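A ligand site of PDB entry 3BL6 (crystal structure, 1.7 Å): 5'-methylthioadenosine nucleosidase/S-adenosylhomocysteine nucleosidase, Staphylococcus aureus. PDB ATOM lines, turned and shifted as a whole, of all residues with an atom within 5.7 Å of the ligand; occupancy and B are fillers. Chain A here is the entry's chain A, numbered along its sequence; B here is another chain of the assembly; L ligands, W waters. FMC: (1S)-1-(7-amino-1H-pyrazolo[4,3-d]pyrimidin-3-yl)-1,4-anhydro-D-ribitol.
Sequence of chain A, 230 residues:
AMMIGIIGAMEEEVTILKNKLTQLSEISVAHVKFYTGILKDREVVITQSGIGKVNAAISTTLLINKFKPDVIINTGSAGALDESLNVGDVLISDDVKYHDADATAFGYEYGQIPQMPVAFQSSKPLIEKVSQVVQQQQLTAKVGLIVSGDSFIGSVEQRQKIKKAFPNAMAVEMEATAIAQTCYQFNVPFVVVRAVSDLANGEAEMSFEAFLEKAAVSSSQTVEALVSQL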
ATOM      1  N   ALA A   9      19.960  34.984  12.572  1.00  0.00           N
ATOM      2  CA  ALA A   9      18.593  34.481  12.467  1.00  0.00           C
ATOM      3  C   ALA A   9      17.766  34.915  13.670  1.00  0.00           C
ATOM      4  O   ALA A   9      16.611  35.311  13.526  1.00  0.00           O
ATOM      5  CB  ALA A   9      18.578  32.991  12.348  1.00  0.00           C
ATOM      6  N   MET A  10      18.374  34.820  14.837  1.00  0.00           N
ATOM      7  CA  MET A  10      17.682  34.868  16.106  1.00  0.00           C
ATOM      8  C   MET A  10      18.142  36.102  16.884  1.00  0.00           C
ATOM      9  O   MET A  10      19.275  36.545  16.760  1.00  0.00           O
ATOM     10  CB  MET A  10      17.998  33.615  16.917  1.00  0.00           C
ATOM     11  CG  MET A  10      17.418  32.306  16.362  1.00  0.00           C
ATOM     12  SD  MET A  10      18.074  30.842  17.182  1.00  0.00           S
ATOM     13  CE  MET A  10      17.181  29.519  16.392  1.00  0.00           C
ATOM     14  N   GLU A  13      21.315  35.836  18.698  1.00  0.00           N
ATOM     15  CA  GLU A  13      22.512  35.847  17.870  1.00  0.00           C
ATOM     16  C   GLU A  13      22.948  37.245  17.439  1.00  0.00           C
ATOM     17  O   GLU A  13      24.091  37.430  17.026  1.00  0.00           O
ATOM     18  CB  GLU A  13      22.316  34.953  16.644  1.00  0.00           C
ATOM     19  CG  GLU A  13      22.008  33.489  16.996  1.00  0.00           C
ATOM     20  CD  GLU A  13      21.563  32.676  15.801  1.00  0.00           C
ATOM     21  OE1 GLU A  13      20.730  33.185  15.025  1.00  0.00           O
ATOM     22  OE2 GLU A  13      22.038  31.534  15.642  1.00  0.00           O
ATOM     23  N   GLY A  50      15.328  35.688  10.865  1.00  0.00           N
ATOM     24  CA  GLY A  50      14.330  34.655  11.059  1.00  0.00           C
ATOM     25  C   GLY A  50      15.082  33.420  10.592  1.00  0.00           C
ATOM     26  O   GLY A  50      16.169  33.534  10.006  1.00  0.00           O
ATOM     27  N   ILE A  51      14.514  32.236  10.821  1.00  0.00           N
ATOM     28  CA  ILE A  51      15.170  30.974  10.481  1.00  0.00           C
ATOM     29  C   ILE A  51      14.812  30.365   9.131  1.00  0.00           C
ATOM     30  O   ILE A  51      13.694  30.535   8.634  1.00  0.00           O
ATOM     31  CB  ILE A  51      14.881  29.937  11.601  1.00  0.00           C
ATOM     32  CG1 ILE A  51      15.429  30.463  12.937  1.00  0.00           C
ATOM     33  CG2 ILE A  51      15.506  28.583  11.270  1.00  0.00           C
ATOM     34  CD1 ILE A  51      14.870  29.784  14.180  1.00  0.00           C
ATOM     35  N   GLY A  52      15.777  29.650   8.540  1.00  0.00           N
ATOM     36  CA  GLY A  52      15.542  28.979   7.269  1.00  0.00           C
ATOM     37  C   GLY A  52      15.890  29.733   5.996  1.00  0.00           C
ATOM     38  O   GLY A  52      16.142  30.947   6.015  1.00  0.00           O
ATOM     39  N   SER A  77      24.769  30.359  14.944  1.00  0.00           N
ATOM     40  CA  SER A  77      25.319  29.055  15.348  1.00  0.00           C
ATOM     41  C   SER A  77      25.271  28.032  14.213  1.00  0.00           C
ATOM     42  O   SER A  77      24.791  28.320  13.131  1.00  0.00           O
ATOM     43  CB  SER A  77      24.533  28.508  16.546  1.00  0.00           C
ATOM     44  OG  SER A  77      23.238  28.096  16.158  1.00  0.00           O
ATOM     45  N   ALA A  78      25.774  26.837  14.485  1.00  0.00           N
ATOM     46  CA  ALA A  78      25.773  25.760  13.505  1.00  0.00           C
ATOM     47  C   ALA A  78      26.159  24.453  14.206  1.00  0.00           C
ATOM     48  O   ALA A  78      26.731  24.475  15.290  1.00  0.00           O
ATOM     49  CB  ALA A  78      26.752  26.047  12.380  1.00  0.00           C
ATOM     50  N   GLY A  79      25.839  23.330  13.567  1.00  0.00           N
ATOM     51  CA  GLY A  79      26.195  22.029  14.125  1.00  0.00           C
ATOM     52  C   GLY A  79      27.499  21.572  13.501  1.00  0.00           C
ATOM     53  O   GLY A  79      27.669  21.665  12.285  1.00  0.00           O
ATOM     54  N   SER A 151      16.286  22.041   7.489  1.00  0.00           N
ATOM     55  CA  SER A 151      16.071  21.070   8.553  1.00  0.00           C
ATOM     56  C   SER A 151      17.117  21.236   9.664  1.00  0.00           C
ATOM     57  O   SER A 151      18.236  21.698   9.411  1.00  0.00           O
ATOM     58  CB  SER A 151      16.162  19.641   8.008  1.00  0.00           C
ATOM     59  OG  SER A 151      15.166  19.388   7.035  1.00  0.00           O
ATOM     60  N   PHE A 152      16.740  20.889  10.887  1.00  0.00           N
ATOM     61  CA  PHE A 152      17.681  20.955  11.986  1.00  0.00           C
ATOM     62  C   PHE A 152      18.299  19.566  12.009  1.00  0.00           C
ATOM     63  O   PHE A 152      17.575  18.563  12.029  1.00  0.00           O
ATOM     64  CB  PHE A 152      16.976  21.225  13.320  1.00  0.00           C
ATOM     65  CG  PHE A 152      17.906  21.282  14.492  1.00  0.00           C
ATOM     66  CD1 PHE A 152      18.665  22.421  14.742  1.00  0.00           C
ATOM     67  CD2 PHE A 152      18.063  20.177  15.337  1.00  0.00           C
ATOM     68  CE1 PHE A 152      19.559  22.470  15.810  1.00  0.00           C
ATOM     69  CE2 PHE A 152      18.957  20.216  16.406  1.00  0.00           C
ATOM     70  CZ  PHE A 152      19.699  21.361  16.641  1.00  0.00           C
ATOM     71  N   ILE A 153      19.623  19.498  11.983  1.00  0.00           N
ATOM     72  CA  ILE A 153      20.291  18.200  11.989  1.00  0.00           C
ATOM     73  C   ILE A 153      20.477  17.801  13.445  1.00  0.00           C
ATOM     74  O   ILE A 153      21.389  18.277  14.127  1.00  0.00           O
ATOM     75  CB  ILE A 153      21.658  18.286  11.248  1.00  0.00           C
ATOM     76  CG1 ILE A 153      21.469  19.006   9.900  1.00  0.00           C
ATOM     77  CG2 ILE A 153      22.241  16.899  11.041  1.00  0.00           C
ATOM     78  CD1 ILE A 153      20.448  18.393   8.904  1.00  0.00           C
ATOM     79  N   GLY A 154      19.573  16.941  13.920  1.00  0.00           N
ATOM     80  CA  GLY A 154      19.613  16.500  15.295  1.00  0.00           C
ATOM     81  C   GLY A 154      19.557  14.994  15.475  1.00  0.00           C
ATOM     82  O   GLY A 154      18.926  14.505  16.404  1.00  0.00           O
ATOM     83  N   VAL A 172      26.978  22.461   9.615  1.00  0.00           N
ATOM     84  CA  VAL A 172      25.666  22.523   8.958  1.00  0.00           C
ATOM     85  C   VAL A 172      24.738  23.478   9.700  1.00  0.00           C
ATOM     86  O   VAL A 172      24.728  23.538  10.927  1.00  0.00           O
ATOM     87  CB  VAL A 172      25.008  21.105   8.892  1.00  0.00           C
ATOM     88  CG1 VAL A 172      24.844  20.537  10.304  1.00  0.00           C
ATOM     89  CG2 VAL A 172      23.638  21.189   8.202  1.00  0.00           C
ATOM     90  N   GLU A 173      23.971  24.256   8.945  1.00  0.00           N
ATOM     91  CA  GLU A 173      23.015  25.157   9.553  1.00  0.00           C
ATOM     92  C   GLU A 173      21.938  25.551   8.530  1.00  0.00           C
ATOM     93  O   GLU A 173      21.946  25.040   7.409  1.00  0.00           O
ATOM     94  CB  GLU A 173      23.706  26.428  10.087  1.00  0.00           C
ATOM     95  CG  GLU A 173      24.764  27.018   9.181  1.00  0.00           C
ATOM     96  CD  GLU A 173      24.160  27.533   7.913  1.00  0.00           C
ATOM     97  OE1 GLU A 173      23.606  28.651   7.945  1.00  0.00           O
ATOM     98  OE2 GLU A 173      24.200  26.807   6.894  1.00  0.00           O
ATOM     99  N   MET A 174      21.027  26.463   8.871  1.00  0.00           N
ATOM    100  CA  MET A 174      19.927  26.740   7.947  1.00  0.00           C
ATOM    101  C   MET A 174      19.891  27.914   6.980  1.00  0.00           C
ATOM    102  O   MET A 174      19.141  27.879   6.011  1.00  0.00           O
ATOM    103  CB  MET A 174      18.694  26.564   8.844  1.00  0.00           C
ATOM    104  CG  MET A 174      18.613  25.198   9.531  1.00  0.00           C
ATOM    105  SD  MET A 174      17.307  25.036  10.803  1.00  0.00           S
ATOM    106  CE  MET A 174      15.821  25.146   9.805  1.00  0.00           C
ATOM    107  N   GLU A 175      20.708  28.952   7.212  1.00  0.00           N
ATOM    108  CA  GLU A 175      20.654  30.093   6.303  1.00  0.00           C
ATOM    109  C   GLU A 175      21.820  30.476   5.398  1.00  0.00           C
ATOM    110  O   GLU A 175      21.619  31.069   4.345  1.00  0.00           O
ATOM    111  CB  GLU A 175      20.379  31.281   7.253  1.00  0.00           C
ATOM    112  CG  GLU A 175      19.115  31.121   8.128  1.00  0.00           C
ATOM    113  CD  GLU A 175      19.363  30.399   9.438  1.00  0.00           C
ATOM    114  OE1 GLU A 175      20.532  30.314   9.874  1.00  0.00           O
ATOM    115  OE2 GLU A 175      18.381  29.919  10.045  1.00  0.00           O
ATOM    116  N   ARG A 194      30.245  32.023  12.058  1.00  0.00           N
ATOM    117  CA  ARG A 194      29.361  31.459  13.058  1.00  0.00           C
ATOM    118  C   ARG A 194      30.171  30.733  14.129  1.00  0.00           C
ATOM    119  O   ARG A 194      31.398  30.809  14.153  1.00  0.00           O
ATOM    120  CB  ARG A 194      28.383  30.475  12.389  1.00  0.00           C
ATOM    121  CG  ARG A 194      27.350  31.153  11.483  1.00  0.00           C
ATOM    122  CD  ARG A 194      26.536  30.129  10.692  1.00  0.00           C
ATOM    123  NE  ARG A 194      25.473  30.740   9.890  1.00  0.00           N
ATOM    124  CZ  ARG A 194      24.187  30.737  10.223  1.00  0.00           C
ATOM    125  NH1 ARG A 194      23.778  30.161  11.357  1.00  0.00           N
ATOM    126  NH2 ARG A 194      23.282  31.310   9.434  1.00  0.00           N
ATOM    127  N   SER A 197      27.368  25.322  18.238  1.00  0.00           N
ATOM    128  CA  SER A 197      26.422  25.297  19.334  1.00  0.00           C
ATOM    129  C   SER A 197      26.097  23.840  19.671  1.00  0.00           C
ATOM    130  O   SER A 197      25.596  23.542  20.739  1.00  0.00           O
ATOM    131  CB  SER A 197      25.127  26.044  18.967  1.00  0.00           C
ATOM    132  OG  SER A 197      24.548  25.499  17.782  1.00  0.00           O
ATOM    133  N   ASP A 198      26.428  22.942  18.743  1.00  0.00           N
ATOM    134  CA  ASP A 198      26.118  21.532  18.919  1.00  0.00           C
ATOM    135  C   ASP A 198      26.885  20.669  17.911  1.00  0.00           C
ATOM    136  O   ASP A 198      27.522  21.201  16.994  1.00  0.00           O
ATOM    137  CB  ASP A 198      24.604  21.334  18.746  1.00  0.00           C
ATOM    138  CG  ASP A 198      24.115  21.788  17.370  1.00  0.00           C
ATOM    139  OD1 ASP A 198      24.186  20.974  16.421  1.00  0.00           O
ATOM    140  OD2 ASP A 198      23.685  22.959  17.236  1.00  0.00           O
ATOM    141  N   LEU A 199      26.816  19.353  18.084  1.00  0.00           N
ATOM    142  CA  LEU A 199      27.528  18.435  17.199  1.00  0.00           C
ATOM    143  C   LEU A 199      26.620  17.772  16.162  1.00  0.00           C
ATOM    144  O   LEU A 199      26.986  16.766  15.561  1.00  0.00           O
ATOM    145  CB  LEU A 199      28.249  17.361  18.030  1.00  0.00           C
ATOM    146  CG  LEU A 199      29.113  17.889  19.190  1.00  0.00           C
ATOM    147  CD1 LEU A 199      29.924  16.729  19.761  1.00  0.00           C
ATOM    148  CD2 LEU A 199      30.050  18.994  18.710  1.00  0.00           C
ATOM    149  N   ALA A 200      25.441  18.360  15.961  1.00  0.00           N
ATOM    150  CA  ALA A 200      24.474  17.865  14.985  1.00  0.00           C
ATOM    151  C   ALA A 200      24.306  16.351  15.161  1.00  0.00           C
ATOM    152  O   ALA A 200      24.480  15.602  14.198  1.00  0.00           O
ATOM    153  CB  ALA A 200      24.995  18.119  13.571  1.00  0.00           C
ATOM    154  N   ALA A 204      21.978  17.083  19.717  1.00  0.00           N
ATOM    155  CA  ALA A 204      22.018  18.409  19.110  1.00  0.00           C
ATOM    156  C   ALA A 204      21.013  19.403  19.679  1.00  0.00           C
ATOM    157  O   ALA A 204      21.367  20.529  20.002  1.00  0.00           O
ATOM    158  CB  ALA A 204      21.867  18.294  17.599  1.00  0.00           C
ATOM    159  N   PHE A 208      22.197  22.577  21.687  1.00  0.00           N
ATOM    160  CA  PHE A 208      21.840  23.891  21.149  1.00  0.00           C
ATOM    161  C   PHE A 208      21.312  24.798  22.275  1.00  0.00           C
ATOM    162  O   PHE A 208      21.731  25.947  22.398  1.00  0.00           O
ATOM    163  CB  PHE A 208      20.760  23.747  20.060  1.00  0.00           C
ATOM    164  CG  PHE A 208      20.279  25.059  19.490  1.00  0.00           C
ATOM    165  CD1 PHE A 208      20.941  25.637  18.408  1.00  0.00           C
ATOM    166  CD2 PHE A 208      19.188  25.711  20.048  1.00  0.00           C
ATOM    167  CE1 PHE A 208      20.518  26.860  17.896  1.00  0.00           C
ATOM    168  CE2 PHE A 208      18.755  26.943  19.538  1.00  0.00           C
ATOM    169  CZ  PHE A 208      19.427  27.512  18.454  1.00  0.00           C
ATOM    170  N   PHE B 106      12.740  20.323  17.688  1.00  0.00           N
ATOM    171  CA  PHE B 106      12.335  21.379  18.620  1.00  0.00           C
ATOM    172  C   PHE B 106      10.831  21.282  18.957  1.00  0.00           C
ATOM    173  O   PHE B 106      10.315  22.107  19.693  1.00  0.00           O
ATOM    174  CB  PHE B 106      12.622  22.753  18.027  1.00  0.00           C
ATOM    175  CG  PHE B 106      14.089  23.086  17.918  1.00  0.00           C
ATOM    176  CD1 PHE B 106      14.846  23.332  19.067  1.00  0.00           C
ATOM    177  CD2 PHE B 106      14.699  23.181  16.683  1.00  0.00           C
ATOM    178  CE1 PHE B 106      16.201  23.662  18.977  1.00  0.00           C
ATOM    179  CE2 PHE B 106      16.058  23.519  16.577  1.00  0.00           C
ATOM    180  CZ  PHE B 106      16.802  23.753  17.723  1.00  0.00           C
ATOM    181  N   PRO B 114      10.769  26.895  11.862  1.00  0.00           N
ATOM    182  CA  PRO B 114      10.709  27.438  13.211  1.00  0.00           C
ATOM    183  C   PRO B 114      10.115  28.828  13.244  1.00  0.00           C
ATOM    184  O   PRO B 114      10.508  29.715  12.483  1.00  0.00           O
ATOM    185  CB  PRO B 114      12.177  27.442  13.652  1.00  0.00           C
ATOM    186  CG  PRO B 114      12.729  26.260  12.955  1.00  0.00           C
ATOM    187  CD  PRO B 114      12.042  26.211  11.616  1.00  0.00           C
HETATM  188  N1  FMC L   1      21.384  21.847  12.261  1.00  0.00           N
HETATM  189  C2  FMC L   1      20.757  22.846  11.569  1.00  0.00           C
HETATM  190  N3  FMC L   1      20.749  24.147  11.911  1.00  0.00           N
HETATM  191  C4  FMC L   1      21.497  24.441  13.111  1.00  0.00           C
HETATM  192  C5  FMC L   1      22.173  23.464  13.865  1.00  0.00           C
HETATM  193  C6  FMC L   1      22.101  22.081  13.418  1.00  0.00           C
HETATM  194  N6  FMC L   1      22.688  21.083  14.072  1.00  0.00           N
HETATM  195  N7  FMC L   1      22.766  24.083  14.930  1.00  0.00           N
HETATM  196  N8  FMC L   1      22.499  25.439  14.889  1.00  0.00           N
HETATM  197  C9  FMC L   1      21.748  25.692  13.813  1.00  0.00           C
HETATM  198  C1' FMC L   1      21.235  27.104  13.439  1.00  0.00           C
HETATM  199  C2' FMC L   1      20.397  27.357  12.146  1.00  0.00           C
HETATM  200  O2' FMC L   1      21.009  28.124  11.118  1.00  0.00           O
HETATM  201  C3' FMC L   1      19.101  27.966  12.637  1.00  0.00           C
HETATM  202  O3' FMC L   1      19.206  29.385  12.396  1.00  0.00           O
HETATM  203  C4' FMC L   1      18.950  27.627  14.146  1.00  0.00           C
HETATM  204  O4' FMC L   1      20.378  27.579  14.525  1.00  0.00           O
HETATM  205  C5' FMC L   1      18.262  26.226  14.457  1.00  0.00           C
HETATM  206  O5' FMC L   1      16.878  26.123  14.130  1.00  0.00           O
HETATM  207  O   HOH W   1      20.627  29.514  16.480  1.00  0.00           O
HETATM  208  O   HOH W   2      21.471  30.704  13.093  1.00  0.00           O
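Residues that only touch the ligand: Glu 173 (3.3 Å), Phe 152 (3.4 Å), Met 10 (3.4 Å), Phe 208 (3.4 Å), Ala 78 (3.5 Å), Ser 151 (3.5 Å), Ser 197 (3.5 Å), Ala 9 (3.7 Å), Phe 106 of chain B (3.7 Å), Ala 200 (3.8 Å), Val 172 (3.9 Å) and Ile 51 (3.9 Å). Hydrophobic or aromatic side chains that line the ligand: Ala 9, Met 10, Ile 51, Phe 152, Ile 153, Met 174, Ala 200, Phe 208 and Phe 106 of chain B.
Water W2 lies within hydrogen-bond range of an oxygen (O3') of the ligand (2.7 Å), the side-chain carboxylate of Glu 13 (2.7 Å), the guanidinium group of Arg 194 (2.9 Å) and the side-chain carboxylate of Glu 175 (3.4 Å).
The backbone NH (N) of Gly 50 is in hydrogen-bond range of the backbone carbonyl oxygen (O) of Ala 9, 3.0 Å away. OG of Ser 197 lies close to OG of Ser 77 (3.3 Å). OD2 of Asp 198 is in hydrogen-bond range of OG of Ser 197, at 2.7 Å. The backbone NH of Ser 197 is in hydrogen-bond range of the backbone carbonyl oxygen of Ala 78, at 3.1 Å. The backbone NH of Ser 77 is in hydrogen-bond range of the side-chain carboxylate of Glu 13, 3.1 Å away. The backbone NH of Glu 175 lies within hydrogen-bond range of the side-chain carboxylate of Glu 173 (3.0 Å). O of Ser 77 is in hydrogen-bond range of NH1 of Arg 194, at 2.8 Å. The side-chain carboxylate (OE1) of Glu 175 lies within salt-bridge range of the guanidinium group (NH2) of Arg 194, at 3.0 Å.
O2' of the ligand sits at hydrogen-bond distance from N of Met 174 (2.8 Å). The backbone NH (N) of Gly 79 lies close to a nitrogen (N7) of the ligand (3.4 Å). The backbone NH (N) of Ile 153 sits at hydrogen-bond distance from a nitrogen (N1) of the ligand (2.9 Å). OG of Ser 77 is in hydrogen-bond range of N8 of the ligand (3.0 Å). The side-chain sulfur of Met 174 sits at hydrogen-bond distance from an oxygen (O5') of the ligand (3.5 Å). O2' of the ligand sits at hydrogen-bond distance from NH1 of Arg 194, 3.4 Å away. The backbone carbonyl oxygen (O) of Ile 153 sits at hydrogen-bond distance from a nitrogen (N6) of the ligand (3.1 Å). The side-chain carboxylate (OD2) of Asp 198 is in hydrogen-bond range of a nitrogen (N7) of the ligand (2.7 Å). O3' of the ligand lies within hydrogen-bond range of OE2 of Glu 175 (2.5 Å).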
